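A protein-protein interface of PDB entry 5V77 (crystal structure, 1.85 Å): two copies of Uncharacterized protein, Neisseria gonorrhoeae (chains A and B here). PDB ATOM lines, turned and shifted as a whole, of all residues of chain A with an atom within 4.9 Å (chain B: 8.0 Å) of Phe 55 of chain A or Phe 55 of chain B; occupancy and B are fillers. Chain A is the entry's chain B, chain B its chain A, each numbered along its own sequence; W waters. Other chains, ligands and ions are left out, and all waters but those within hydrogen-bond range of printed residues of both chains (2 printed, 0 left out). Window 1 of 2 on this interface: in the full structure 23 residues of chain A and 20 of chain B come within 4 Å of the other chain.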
ATOM      1  N   ILE A  22     -12.613   5.756 -11.820  1.00  0.00           N
ATOM      2  CA  ILE A  22     -11.896   6.096 -13.044  1.00  0.00           C
ATOM      3  C   ILE A  22     -11.800   4.806 -13.845  1.00  0.00           C
ATOM      4  O   ILE A  22     -11.201   3.831 -13.374  1.00  0.00           O
ATOM      5  CB  ILE A  22     -10.491   6.648 -12.737  1.00  0.00           C
ATOM      6  CG1 ILE A  22     -10.580   7.917 -11.872  1.00  0.00           C
ATOM      7  CG2 ILE A  22      -9.732   6.946 -14.019  1.00  0.00           C
ATOM      8  CD1 ILE A  22      -9.236   8.357 -11.318  1.00  0.00           C
ATOM      9  N   PHE A  24     -11.173   2.712 -17.540  1.00  0.00           N
ATOM     10  CA  PHE A  24     -10.791   2.568 -18.941  1.00  0.00           C
ATOM     11  C   PHE A  24     -11.866   1.813 -19.707  1.00  0.00           C
ATOM     12  O   PHE A  24     -12.433   0.845 -19.202  1.00  0.00           O
ATOM     13  CB  PHE A  24      -9.484   1.770 -19.091  1.00  0.00           C
ATOM     14  CG  PHE A  24      -8.255   2.538 -18.725  1.00  0.00           C
ATOM     15  CD1 PHE A  24      -7.606   3.318 -19.678  1.00  0.00           C
ATOM     16  CD2 PHE A  24      -7.730   2.453 -17.442  1.00  0.00           C
ATOM     17  CE1 PHE A  24      -6.456   4.013 -19.349  1.00  0.00           C
ATOM     18  CE2 PHE A  24      -6.588   3.138 -17.101  1.00  0.00           C
ATOM     19  CZ  PHE A  24      -5.948   3.933 -18.060  1.00  0.00           C
ATOM     20  N   LEU A  31     -11.214   7.109 -21.184  1.00  0.00           N
ATOM     21  CA  LEU A  31     -11.239   7.107 -19.729  1.00  0.00           C
ATOM     22  C   LEU A  31     -12.484   7.848 -19.282  1.00  0.00           C
ATOM     23  O   LEU A  31     -12.710   8.983 -19.715  1.00  0.00           O
ATOM     24  CB  LEU A  31     -10.012   7.809 -19.159  1.00  0.00           C
ATOM     25  CG  LEU A  31      -8.792   7.017 -18.743  1.00  0.00           C
ATOM     26  CD1 LEU A  31      -7.784   8.010 -18.250  1.00  0.00           C
ATOM     27  CD2 LEU A  31      -9.164   6.018 -17.659  1.00  0.00           C
ATOM     28  N   ILE A  52      -6.766   9.081 -25.412  1.00  0.00           N
ATOM     29  CA  ILE A  52      -5.935   9.578 -24.329  1.00  0.00           C
ATOM     30  C   ILE A  52      -4.549   9.906 -24.850  1.00  0.00           C
ATOM     31  O   ILE A  52      -3.963   9.158 -25.645  1.00  0.00           O
ATOM     32  CB  ILE A  52      -5.850   8.538 -23.199  1.00  0.00           C
ATOM     33  CG1 ILE A  52      -7.247   8.182 -22.697  1.00  0.00           C
ATOM     34  CG2 ILE A  52      -4.985   9.058 -22.071  1.00  0.00           C
ATOM     35  CD1 ILE A  52      -7.988   9.353 -22.113  1.00  0.00           C
ATOM     36  N   LEU A  53      -4.015  11.034 -24.396  1.00  0.00           N
ATOM     37  CA  LEU A  53      -2.631  11.405 -24.649  1.00  0.00           C
ATOM     38  C   LEU A  53      -1.768  11.145 -23.423  1.00  0.00           C
ATOM     39  O   LEU A  53      -0.741  10.466 -23.514  1.00  0.00           O
ATOM     40  CB  LEU A  53      -2.550  12.881 -25.073  1.00  0.00           C
ATOM     41  CG  LEU A  53      -3.390  13.233 -26.299  1.00  0.00           C
ATOM     42  CD1 LEU A  53      -3.413  14.742 -26.509  1.00  0.00           C
ATOM     43  CD2 LEU A  53      -2.871  12.524 -27.551  1.00  0.00           C
ATOM     44  N   ASN A  54      -2.170  11.646 -22.258  1.00  0.00           N
ATOM     45  CA  ASN A  54      -1.490  11.236 -21.040  1.00  0.00           C
ATOM     46  C   ASN A  54      -2.443  11.315 -19.857  1.00  0.00           C
ATOM     47  O   ASN A  54      -3.413  12.075 -19.859  1.00  0.00           O
ATOM     48  CB  ASN A  54      -0.234  12.067 -20.767  1.00  0.00           C
ATOM     49  CG  ASN A  54      -0.485  13.543 -20.886  1.00  0.00           C
ATOM     50  OD1 ASN A  54      -1.068  14.154 -19.992  1.00  0.00           O
ATOM     51  ND2 ASN A  54      -0.049  14.134 -21.995  1.00  0.00           N
ATOM     52  N   PHE A  55      -2.148  10.484 -18.860  1.00  0.00           N
ATOM     53  CA  PHE A  55      -2.899  10.416 -17.616  1.00  0.00           C
ATOM     54  C   PHE A  55      -1.882  10.341 -16.495  1.00  0.00           C
ATOM     55  O   PHE A  55      -0.953   9.527 -16.539  1.00  0.00           O
ATOM     56  CB  PHE A  55      -3.838   9.199 -17.552  1.00  0.00           C
ATOM     57  CG  PHE A  55      -4.446   8.971 -16.180  1.00  0.00           C
ATOM     58  CD1 PHE A  55      -5.728   9.373 -15.911  1.00  0.00           C
ATOM     59  CD2 PHE A  55      -3.721   8.361 -15.164  1.00  0.00           C
ATOM     60  CE1 PHE A  55      -6.291   9.186 -14.670  1.00  0.00           C
ATOM     61  CE2 PHE A  55      -4.271   8.167 -13.918  1.00  0.00           C
ATOM     62  CZ  PHE A  55      -5.563   8.579 -13.669  1.00  0.00           C
ATOM     63  N   LYS A  56      -2.026  11.216 -15.512  1.00  0.00           N
ATOM     64  CA  LYS A  56      -1.150  11.196 -14.351  1.00  0.00           C
ATOM     65  C   LYS A  56      -2.004  11.267 -13.102  1.00  0.00           C
ATOM     66  O   LYS A  56      -2.923  12.087 -13.025  1.00  0.00           O
ATOM     67  CB  LYS A  56      -0.152  12.363 -14.370  1.00  0.00           C
ATOM     68  N   LEU A  57      -1.705  10.397 -12.138  1.00  0.00           N
ATOM     69  CA  LEU A  57      -2.290  10.457 -10.808  1.00  0.00           C
ATOM     70  C   LEU A  57      -1.121  10.466  -9.840  1.00  0.00           C
ATOM     71  O   LEU A  57      -0.248   9.602  -9.926  1.00  0.00           O
ATOM     72  CB  LEU A  57      -3.224   9.260 -10.533  1.00  0.00           C
ATOM     73  CG  LEU A  57      -3.428   8.890  -9.045  1.00  0.00           C
ATOM     74  CD1 LEU A  57      -4.210   9.940  -8.316  1.00  0.00           C
ATOM     75  CD2 LEU A  57      -4.096   7.526  -8.885  1.00  0.00           C
ATOM     76  N   ILE A  99      -4.680  14.866 -10.304  1.00  0.00           N
ATOM     77  CA  ILE A  99      -5.014  14.056 -11.472  1.00  0.00           C
ATOM     78  C   ILE A  99      -5.002  14.985 -12.672  1.00  0.00           C
ATOM     79  O   ILE A  99      -5.657  16.033 -12.648  1.00  0.00           O
ATOM     80  CB  ILE A  99      -6.391  13.383 -11.331  1.00  0.00           C
ATOM     81  CG1 ILE A  99      -6.387  12.352 -10.191  1.00  0.00           C
ATOM     82  CG2 ILE A  99      -6.827  12.736 -12.674  1.00  0.00           C
ATOM     83  CD1 ILE A  99      -7.780  11.888  -9.805  1.00  0.00           C
ATOM     84  N   LYS A 100      -4.256  14.614 -13.711  1.00  0.00           N
ATOM     85  CA  LYS A 100      -4.228  15.388 -14.948  1.00  0.00           C
ATOM     86  C   LYS A 100      -4.443  14.428 -16.098  1.00  0.00           C
ATOM     87  O   LYS A 100      -3.772  13.395 -16.174  1.00  0.00           O
ATOM     88  CB  LYS A 100      -2.900  16.123 -15.159  1.00  0.00           C
ATOM     89  CG  LYS A 100      -2.488  17.059 -14.056  1.00  0.00           C
ATOM     90  CD  LYS A 100      -1.162  17.722 -14.434  1.00  0.00           C
ATOM     91  CE  LYS A 100      -0.664  18.652 -13.338  1.00  0.00           C
ATOM     92  NZ  LYS A 100       0.744  19.067 -13.602  1.00  0.00           N
ATOM     93  N   ILE A 101      -5.365  14.765 -16.991  1.00  0.00           N
ATOM     94  CA  ILE A 101      -5.656  13.932 -18.153  1.00  0.00           C
ATOM     95  C   ILE A 101      -5.721  14.832 -19.371  1.00  0.00           C
ATOM     96  O   ILE A 101      -6.524  15.767 -19.402  1.00  0.00           O
ATOM     97  CB  ILE A 101      -6.984  13.171 -17.999  1.00  0.00           C
ATOM     98  CG1 ILE A 101      -7.023  12.414 -16.669  1.00  0.00           C
ATOM     99  CG2 ILE A 101      -7.181  12.219 -19.188  1.00  0.00           C
ATOM    100  CD1 ILE A 101      -8.316  11.621 -16.446  1.00  0.00           C
ATOM    101  N   LEU B  19      -1.238  -6.973 -21.811  1.00  0.00           N
ATOM    102  CA  LEU B  19      -2.043  -6.233 -20.844  1.00  0.00           C
ATOM    103  C   LEU B  19      -3.415  -5.910 -21.429  1.00  0.00           C
ATOM    104  O   LEU B  19      -3.511  -5.322 -22.511  1.00  0.00           O
ATOM    105  CB  LEU B  19      -1.325  -4.945 -20.456  1.00  0.00           C
ATOM    106  CG  LEU B  19      -2.114  -3.974 -19.569  1.00  0.00           C
ATOM    107  CD1 LEU B  19      -2.234  -4.569 -18.181  1.00  0.00           C
ATOM    108  CD2 LEU B  19      -1.376  -2.664 -19.519  1.00  0.00           C
ATOM    109  N   ILE B  22      -6.615  -2.247 -16.633  1.00  0.00           N
ATOM    110  CA  ILE B  22      -5.998  -1.545 -15.512  1.00  0.00           C
ATOM    111  C   ILE B  22      -7.148  -1.112 -14.622  1.00  0.00           C
ATOM    112  O   ILE B  22      -8.006  -0.346 -15.063  1.00  0.00           O
ATOM    113  CB  ILE B  22      -5.187  -0.319 -15.969  1.00  0.00           C
ATOM    114  CG1 ILE B  22      -4.047  -0.737 -16.916  1.00  0.00           C
ATOM    115  CG2 ILE B  22      -4.641   0.428 -14.761  1.00  0.00           C
ATOM    116  CD1 ILE B  22      -3.348   0.454 -17.553  1.00  0.00           C
ATOM    117  N   ILE B  23      -7.211  -1.638 -13.404  1.00  0.00           N
ATOM    118  CA  ILE B  23      -8.431  -1.565 -12.596  1.00  0.00           C
ATOM    119  C   ILE B  23      -8.108  -0.992 -11.226  1.00  0.00           C
ATOM    120  O   ILE B  23      -7.251  -1.524 -10.520  1.00  0.00           O
ATOM    121  CB  ILE B  23      -9.067  -2.957 -12.443  1.00  0.00           C
ATOM    122  CG1 ILE B  23      -9.411  -3.518 -13.831  1.00  0.00           C
ATOM    123  CG2 ILE B  23     -10.262  -2.905 -11.508  1.00  0.00           C
ATOM    124  CD1 ILE B  23     -10.498  -2.730 -14.551  1.00  0.00           C
ATOM    125  N   PHE B  24      -8.850   0.039 -10.814  1.00  0.00           N
ATOM    126  CA  PHE B  24      -8.761   0.523  -9.437  1.00  0.00           C
ATOM    127  C   PHE B  24      -9.566  -0.378  -8.501  1.00  0.00           C
ATOM    128  O   PHE B  24     -10.685  -0.780  -8.833  1.00  0.00           O
ATOM    129  CB  PHE B  24      -9.319   1.953  -9.342  1.00  0.00           C
ATOM    130  CG  PHE B  24      -8.366   3.021  -9.796  1.00  0.00           C
ATOM    131  CD1 PHE B  24      -7.411   3.528  -8.922  1.00  0.00           C
ATOM    132  CD2 PHE B  24      -8.444   3.545 -11.076  1.00  0.00           C
ATOM    133  CE1 PHE B  24      -6.534   4.524  -9.331  1.00  0.00           C
ATOM    134  CE2 PHE B  24      -7.563   4.537 -11.493  1.00  0.00           C
ATOM    135  CZ  PHE B  24      -6.612   5.030 -10.608  1.00  0.00           C
ATOM    136  N   LEU B  31      -4.118  -0.515  -7.659  1.00  0.00           N
ATOM    137  CA  LEU B  31      -4.247  -0.715  -9.096  1.00  0.00           C
ATOM    138  C   LEU B  31      -3.845  -2.139  -9.437  1.00  0.00           C
ATOM    139  O   LEU B  31      -2.773  -2.604  -9.018  1.00  0.00           O
ATOM    140  CB  LEU B  31      -3.365   0.259  -9.882  1.00  0.00           C
ATOM    141  CG  LEU B  31      -3.962   1.654 -10.091  1.00  0.00           C
ATOM    142  CD1 LEU B  31      -2.881   2.564 -10.609  1.00  0.00           C
ATOM    143  CD2 LEU B  31      -5.123   1.568 -11.092  1.00  0.00           C
ATOM    144  N   LEU B  33      -3.200  -4.685 -12.722  1.00  0.00           N
ATOM    145  CA  LEU B  33      -3.001  -4.846 -14.153  1.00  0.00           C
ATOM    146  C   LEU B  33      -3.169  -6.321 -14.472  1.00  0.00           C
ATOM    147  O   LEU B  33      -2.560  -7.158 -13.806  1.00  0.00           O
ATOM    148  CB  LEU B  33      -1.604  -4.366 -14.557  1.00  0.00           C
ATOM    149  CG  LEU B  33      -1.393  -2.865 -14.773  1.00  0.00           C
ATOM    150  CD1 LEU B  33      -1.676  -2.079 -13.496  1.00  0.00           C
ATOM    151  CD2 LEU B  33       0.040  -2.596 -15.227  1.00  0.00           C
ATOM    152  N   ILE B  52      -1.160   3.236  -3.846  1.00  0.00           N
ATOM    153  CA  ILE B  52      -0.562   3.906  -4.989  1.00  0.00           C
ATOM    154  C   ILE B  52       0.096   5.205  -4.570  1.00  0.00           C
ATOM    155  O   ILE B  52      -0.483   6.011  -3.824  1.00  0.00           O
ATOM    156  CB  ILE B  52      -1.640   4.174  -6.048  1.00  0.00           C
ATOM    157  CG1 ILE B  52      -2.188   2.843  -6.544  1.00  0.00           C
ATOM    158  CG2 ILE B  52      -1.072   5.015  -7.202  1.00  0.00           C
ATOM    159  CD1 ILE B  52      -1.203   2.031  -7.281  1.00  0.00           C
ATOM    160  N   LEU B  53       1.306   5.426  -5.073  1.00  0.00           N
ATOM    161  CA  LEU B  53       1.988   6.700  -4.937  1.00  0.00           C
ATOM    162  C   LEU B  53       1.812   7.533  -6.192  1.00  0.00           C
ATOM    163  O   LEU B  53       1.314   8.655  -6.114  1.00  0.00           O
ATOM    164  CB  LEU B  53       3.478   6.489  -4.630  1.00  0.00           C
ATOM    165  CG  LEU B  53       3.665   5.629  -3.377  1.00  0.00           C
ATOM    166  CD1 LEU B  53       5.122   5.285  -3.175  1.00  0.00           C
ATOM    167  CD2 LEU B  53       3.102   6.337  -2.164  1.00  0.00           C
ATOM    168  N   ASN B  54       2.174   6.997  -7.356  1.00  0.00           N
ATOM    169  CA  ASN B  54       1.773   7.682  -8.574  1.00  0.00           C
ATOM    170  C   ASN B  54       1.547   6.677  -9.694  1.00  0.00           C
ATOM    171  O   ASN B  54       2.025   5.538  -9.656  1.00  0.00           O
ATOM    172  CB  ASN B  54       2.792   8.742  -8.988  1.00  0.00           C
ATOM    173  CG  ASN B  54       4.190   8.209  -9.008  1.00  0.00           C
ATOM    174  OD1 ASN B  54       4.557   7.449  -9.898  1.00  0.00           O
ATOM    175  ND2 ASN B  54       4.982   8.590  -8.011  1.00  0.00           N
ATOM    176  N   PHE B  55       0.780   7.126 -10.687  1.00  0.00           N
ATOM    177  CA  PHE B  55       0.462   6.342 -11.871  1.00  0.00           C
ATOM    178  C   PHE B  55       0.585   7.272 -13.071  1.00  0.00           C
ATOM    179  O   PHE B  55      -0.046   8.327 -13.093  1.00  0.00           O
ATOM    180  CB  PHE B  55      -0.955   5.750 -11.738  1.00  0.00           C
ATOM    181  CG  PHE B  55      -1.499   5.099 -12.986  1.00  0.00           C
ATOM    182  CD1 PHE B  55      -0.669   4.566 -13.958  1.00  0.00           C
ATOM    183  CD2 PHE B  55      -2.867   5.023 -13.176  1.00  0.00           C
ATOM    184  CE1 PHE B  55      -1.196   3.989 -15.095  1.00  0.00           C
ATOM    185  CE2 PHE B  55      -3.396   4.435 -14.306  1.00  0.00           C
ATOM    186  CZ  PHE B  55      -2.558   3.919 -15.266  1.00  0.00           C
ATOM    187  N   LYS B  56       1.376   6.878 -14.063  1.00  0.00           N
ATOM    188  CA  LYS B  56       1.537   7.676 -15.274  1.00  0.00           C
ATOM    189  C   LYS B  56       1.305   6.792 -16.489  1.00  0.00           C
ATOM    190  O   LYS B  56       1.850   5.688 -16.569  1.00  0.00           O
ATOM    191  CB  LYS B  56       2.931   8.312 -15.338  1.00  0.00           C
ATOM    192  N   LEU B  57       0.474   7.268 -17.409  1.00  0.00           N
ATOM    193  CA  LEU B  57       0.303   6.660 -18.717  1.00  0.00           C
ATOM    194  C   LEU B  57       0.563   7.745 -19.746  1.00  0.00           C
ATOM    195  O   LEU B  57      -0.090   8.787 -19.723  1.00  0.00           O
ATOM    196  CB  LEU B  57      -1.107   6.084 -18.890  1.00  0.00           C
ATOM    197  CG  LEU B  57      -1.527   5.791 -20.339  1.00  0.00           C
ATOM    198  CD1 LEU B  57      -0.761   4.630 -20.886  1.00  0.00           C
ATOM    199  CD2 LEU B  57      -3.017   5.528 -20.429  1.00  0.00           C
ATOM    200  N   ASP B  58       1.515   7.511 -20.641  1.00  0.00           N
ATOM    201  CA  ASP B  58       1.803   8.465 -21.702  1.00  0.00           C
ATOM    202  C   ASP B  58       1.799   7.693 -23.009  1.00  0.00           C
ATOM    203  O   ASP B  58       2.602   6.768 -23.178  1.00  0.00           O
ATOM    204  CB  ASP B  58       3.142   9.163 -21.462  1.00  0.00           C
ATOM    205  CG  ASP B  58       3.475  10.189 -22.529  1.00  0.00           C
ATOM    206  OD1 ASP B  58       2.687  10.381 -23.485  1.00  0.00           O
ATOM    207  OD2 ASP B  58       4.550  10.806 -22.410  1.00  0.00           O
ATOM    208  N   THR B  59       0.895   8.059 -23.928  1.00  0.00           N
ATOM    209  CA  THR B  59       0.820   7.298 -25.171  1.00  0.00           C
ATOM    210  C   THR B  59       1.936   7.663 -26.138  1.00  0.00           C
ATOM    211  O   THR B  59       2.170   6.918 -27.094  1.00  0.00           O
ATOM    212  CB  THR B  59      -0.548   7.464 -25.837  1.00  0.00           C
ATOM    213  OG1 THR B  59      -0.838   8.850 -26.026  1.00  0.00           O
ATOM    214  CG2 THR B  59      -1.621   6.840 -24.959  1.00  0.00           C
ATOM    215  N   LEU B  72      -5.176   1.061 -27.214  1.00  0.00           N
ATOM    216  CA  LEU B  72      -4.214   0.791 -26.152  1.00  0.00           C
ATOM    217  C   LEU B  72      -4.196  -0.689 -25.792  1.00  0.00           C
ATOM    218  O   LEU B  72      -3.136  -1.322 -25.784  1.00  0.00           O
ATOM    219  CB  LEU B  72      -4.546   1.648 -24.936  1.00  0.00           C
ATOM    220  CG  LEU B  72      -3.762   1.387 -23.650  1.00  0.00           C
ATOM    221  CD1 LEU B  72      -2.285   1.675 -23.866  1.00  0.00           C
ATOM    222  CD2 LEU B  72      -4.342   2.244 -22.507  1.00  0.00           C
ATOM    223  N   PHE B  73      -5.361  -1.260 -25.491  1.00  0.00           N
ATOM    224  CA  PHE B  73      -5.545  -2.664 -25.141  1.00  0.00           C
ATOM    225  C   PHE B  73      -6.003  -3.457 -26.358  1.00  0.00           C
ATOM    226  O   PHE B  73      -6.830  -2.972 -27.130  1.00  0.00           O
ATOM    227  CB  PHE B  73      -6.589  -2.830 -24.036  1.00  0.00           C
ATOM    228  CG  PHE B  73      -6.274  -2.082 -22.772  1.00  0.00           C
ATOM    229  CD1 PHE B  73      -4.979  -2.014 -22.275  1.00  0.00           C
ATOM    230  CD2 PHE B  73      -7.289  -1.453 -22.072  1.00  0.00           C
ATOM    231  CE1 PHE B  73      -4.706  -1.320 -21.087  1.00  0.00           C
ATOM    232  CE2 PHE B  73      -7.029  -0.758 -20.889  1.00  0.00           C
ATOM    233  CZ  PHE B  73      -5.745  -0.679 -20.403  1.00  0.00           C
ATOM    234  N   ILE B  91       6.913  -0.278 -11.111  1.00  0.00           N
ATOM    235  CA  ILE B  91       6.994  -1.009 -12.371  1.00  0.00           C
ATOM    236  C   ILE B  91       7.050   0.005 -13.501  1.00  0.00           C
ATOM    237  O   ILE B  91       6.419   1.067 -13.433  1.00  0.00           O
ATOM    238  CB  ILE B  91       5.834  -2.000 -12.588  1.00  0.00           C
ATOM    239  CG1 ILE B  91       4.471  -1.341 -12.361  1.00  0.00           C
ATOM    240  CG2 ILE B  91       6.006  -3.238 -11.712  1.00  0.00           C
ATOM    241  CD1 ILE B  91       3.333  -2.206 -12.872  1.00  0.00           C
ATOM    242  N   ILE B  93       6.629   0.035 -17.749  1.00  0.00           N
ATOM    243  CA  ILE B  93       6.316  -0.606 -19.020  1.00  0.00           C
ATOM    244  C   ILE B  93       6.680   0.385 -20.111  1.00  0.00           C
ATOM    245  O   ILE B  93       6.159   1.503 -20.127  1.00  0.00           O
ATOM    246  CB  ILE B  93       4.831  -0.989 -19.105  1.00  0.00           C
ATOM    247  CG1 ILE B  93       4.469  -2.010 -18.012  1.00  0.00           C
ATOM    248  CG2 ILE B  93       4.498  -1.490 -20.509  1.00  0.00           C
ATOM    249  CD1 ILE B  93       2.974  -2.180 -17.816  1.00  0.00           C
ATOM    250  N   ILE B  98       4.177   4.383 -22.600  1.00  0.00           N
ATOM    251  CA  ILE B  98       4.893   4.228 -21.336  1.00  0.00           C
ATOM    252  C   ILE B  98       3.898   4.250 -20.183  1.00  0.00           C
ATOM    253  O   ILE B  98       3.031   5.127 -20.118  1.00  0.00           O
ATOM    254  CB  ILE B  98       5.962   5.320 -21.156  1.00  0.00           C
ATOM    255  CG1 ILE B  98       7.027   5.168 -22.246  1.00  0.00           C
ATOM    256  CG2 ILE B  98       6.577   5.248 -19.769  1.00  0.00           C
ATOM    257  CD1 ILE B  98       8.284   5.970 -22.012  1.00  0.00           C
ATOM    258  N   ILE B  99       4.028   3.280 -19.279  1.00  0.00           N
ATOM    259  CA  ILE B  99       3.244   3.206 -18.056  1.00  0.00           C
ATOM    260  C   ILE B  99       4.214   3.067 -16.891  1.00  0.00           C
ATOM    261  O   ILE B  99       5.075   2.181 -16.902  1.00  0.00           O
ATOM    262  CB  ILE B  99       2.249   2.028 -18.070  1.00  0.00           C
ATOM    263  CG1 ILE B  99       1.182   2.236 -19.147  1.00  0.00           C
ATOM    264  CG2 ILE B  99       1.578   1.874 -16.671  1.00  0.00           C
ATOM    265  CD1 ILE B  99       0.434   0.961 -19.536  1.00  0.00           C
ATOM    266  N   LYS B 100       4.076   3.934 -15.887  1.00  0.00           N
ATOM    267  CA  LYS B 100       4.895   3.862 -14.680  1.00  0.00           C
ATOM    268  C   LYS B 100       3.958   3.868 -13.487  1.00  0.00           C
ATOM    269  O   LYS B 100       3.050   4.702 -13.420  1.00  0.00           O
ATOM    270  CB  LYS B 100       5.864   5.047 -14.558  1.00  0.00           C
ATOM    271  CG  LYS B 100       6.951   5.134 -15.622  1.00  0.00           C
ATOM    272  CD  LYS B 100       7.957   6.225 -15.243  1.00  0.00           C
ATOM    273  CE  LYS B 100       9.043   6.394 -16.292  1.00  0.00           C
ATOM    274  NZ  LYS B 100      10.002   7.480 -15.931  1.00  0.00           N
ATOM    275  N   ILE B 101       4.156   2.941 -12.557  1.00  0.00           N
ATOM    276  CA  ILE B 101       3.350   2.908 -11.338  1.00  0.00           C
ATOM    277  C   ILE B 101       4.281   2.716 -10.162  1.00  0.00           C
ATOM    278  O   ILE B 101       5.078   1.774 -10.158  1.00  0.00           O
ATOM    279  CB  ILE B 101       2.306   1.776 -11.344  1.00  0.00           C
ATOM    280  CG1 ILE B 101       1.402   1.898 -12.569  1.00  0.00           C
ATOM    281  CG2 ILE B 101       1.461   1.869 -10.053  1.00  0.00           C
ATOM    282  CD1 ILE B 101       0.435   0.736 -12.763  1.00  0.00           C
ATOM    283  N   SER B 102       4.157   3.582  -9.162  1.00  0.00           N
ATOM    284  CA  SER B 102       4.855   3.447  -7.890  1.00  0.00           C
ATOM    285  C   SER B 102       3.821   3.191  -6.801  1.00  0.00           C
ATOM    286  O   SER B 102       2.761   3.820  -6.785  1.00  0.00           O
ATOM    287  CB  SER B 102       5.659   4.707  -7.553  1.00  0.00           C
ATOM    288  OG  SER B 102       6.775   4.848  -8.423  1.00  0.00           O
ATOM    289  N   ALA B 103       4.116   2.250  -5.908  1.00  0.00           N
ATOM    290  CA  ALA B 103       3.152   1.834  -4.891  1.00  0.00           C
ATOM    291  C   ALA B 103       3.927   1.252  -3.717  1.00  0.00           C
ATOM    292  O   ALA B 103       5.050   0.767  -3.883  1.00  0.00           O
ATOM    293  CB  ALA B 103       2.162   0.803  -5.449  1.00  0.00           C
HETATM  294  O   HOH W   1     -10.401   0.769 -15.430  1.00  0.00           O
HETATM  295  O   HOH W   2     -10.743   1.207 -12.857  1.00  0.00           O
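Water W1 bridges the backbone carbonyl oxygen of Ile 22 of chain B (2.7 Å) and the backbone NH of Phe 24 of chain A (3.0 Å). Water W2 bridges the backbone carbonyl oxygen of Ile 22 of chain A (2.7 Å) and the backbone NH of Phe 24 of chain B (3.0 Å).
Among the printed residues, pairs that only touch across the chains: Ile 22 of chain A with Phe 24 of chain B (3.6 Å), Phe 24 of chain A with Ile 22 of chain B (3.7 Å), Phe 24 of chain A with Leu 57 of chain B (3.9 Å), Phe 24 of chain A with Phe 73 of chain B (3.96 Å), Asn 54 of chain A with Leu 57 of chain B (3.1 Å), Phe 55 of chain A with Phe 55 of chain B (3.5 Å), Phe 55 of chain A with Lys 56 of chain B (3.4 Å), Lys 56 of chain A with Phe 55 of chain B (3.3 Å), Leu 57 of chain A with Phe 24 of chain B (3.9 Å) and Leu 57 of chain A with Asn 54 of chain B (3.1 Å).
O of Asn 54 of chain B lies within hydrogen-bond range of N of Ser 102 of chain B, at 2.9 Å. N of Lys 56 of chain B lies within hydrogen-bond range of O of Lys 100 of chain B (2.8 Å). The backbone NH (N) of Asp 58 of chain B lies within hydrogen-bond range of the backbone carbonyl oxygen (O) of Ile 98 of chain B, at 2.9 Å. O of Lys 100 of chain A lies within hydrogen-bond range of N of Lys 56 of chain A.
Of the 24 printed residues of chain B, 9 touch a printed residue of chain A. Hydrophobic or aromatic side chains of chain B within 4 Å of the printed part of chain A: Ile 22, Phe 24, Phe 55, Leu 57 and Phe 73. Among the printed residues, 15 pairs touch across the chains. Among the printed residues, no Asp or Glu carboxylate lies within 4 Å of a Lys or Arg side-chain nitrogen of the other chain.
Ile 22 of chain A touches Phe 24 of chain B, and with the chains exchanged Phe 24 of chain A touches Ile 22 of chain B. Phe 55 of chain B touches its own counterpart, Phe 55 of chain A. Phe 55 of chain A touches Lys 56 of chain B, and with the chains exchanged Lys 56 of chain A touches Phe 55 of chain B. Phe 55 of chain A touches Leu 57 of chain B, and with the chains exchanged Leu 57 of chain A touches Phe 55 of chain B. Of the 15 pairs that touch across the chains among the printed residues, 11 have their exchanged pair printed and touching as well.
Of the printed residues of chain A, Phe 55 of chain B touches Phe 55 (3.5 Å), Lys 56 (3.3 Å) and Leu 57 (2.8 Å). Of the printed residues of chain B, Lys 56 of chain A touches Phe 55 (3.3 Å). Of the printed residues of chain B, Ile 52 of chain A touches Thr 59 (3.2 Å). The nearest printed residue of chain A that does not touch Asp 58 of chain B is Asn 54 of chain A (4.2 Å).
The backbone carbonyl oxygen (O) of Leu 57 of chain B lies within hydrogen-bond range of the backbone NH (N) of Phe 55 of chain A, at 2.8 Å. O of Ile 52 of chain A lies within hydrogen-bond range of OG1 of Thr 59 of chain B (3.2 Å). The side-chain carboxylate of Asp 58 of chain B sits close to the backbone carbonyl oxygen of Leu 53 of chain A (3.4 Å). O of Leu 57 of chain A is in hydrogen-bond range of N of Phe 55 of chain B, 2.8 Å away. The backbone carbonyl oxygen (O) of Leu 53 of chain A lies within hydrogen-bond range of the backbone NH (N) of Thr 59 of chain B (2.9 Å).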
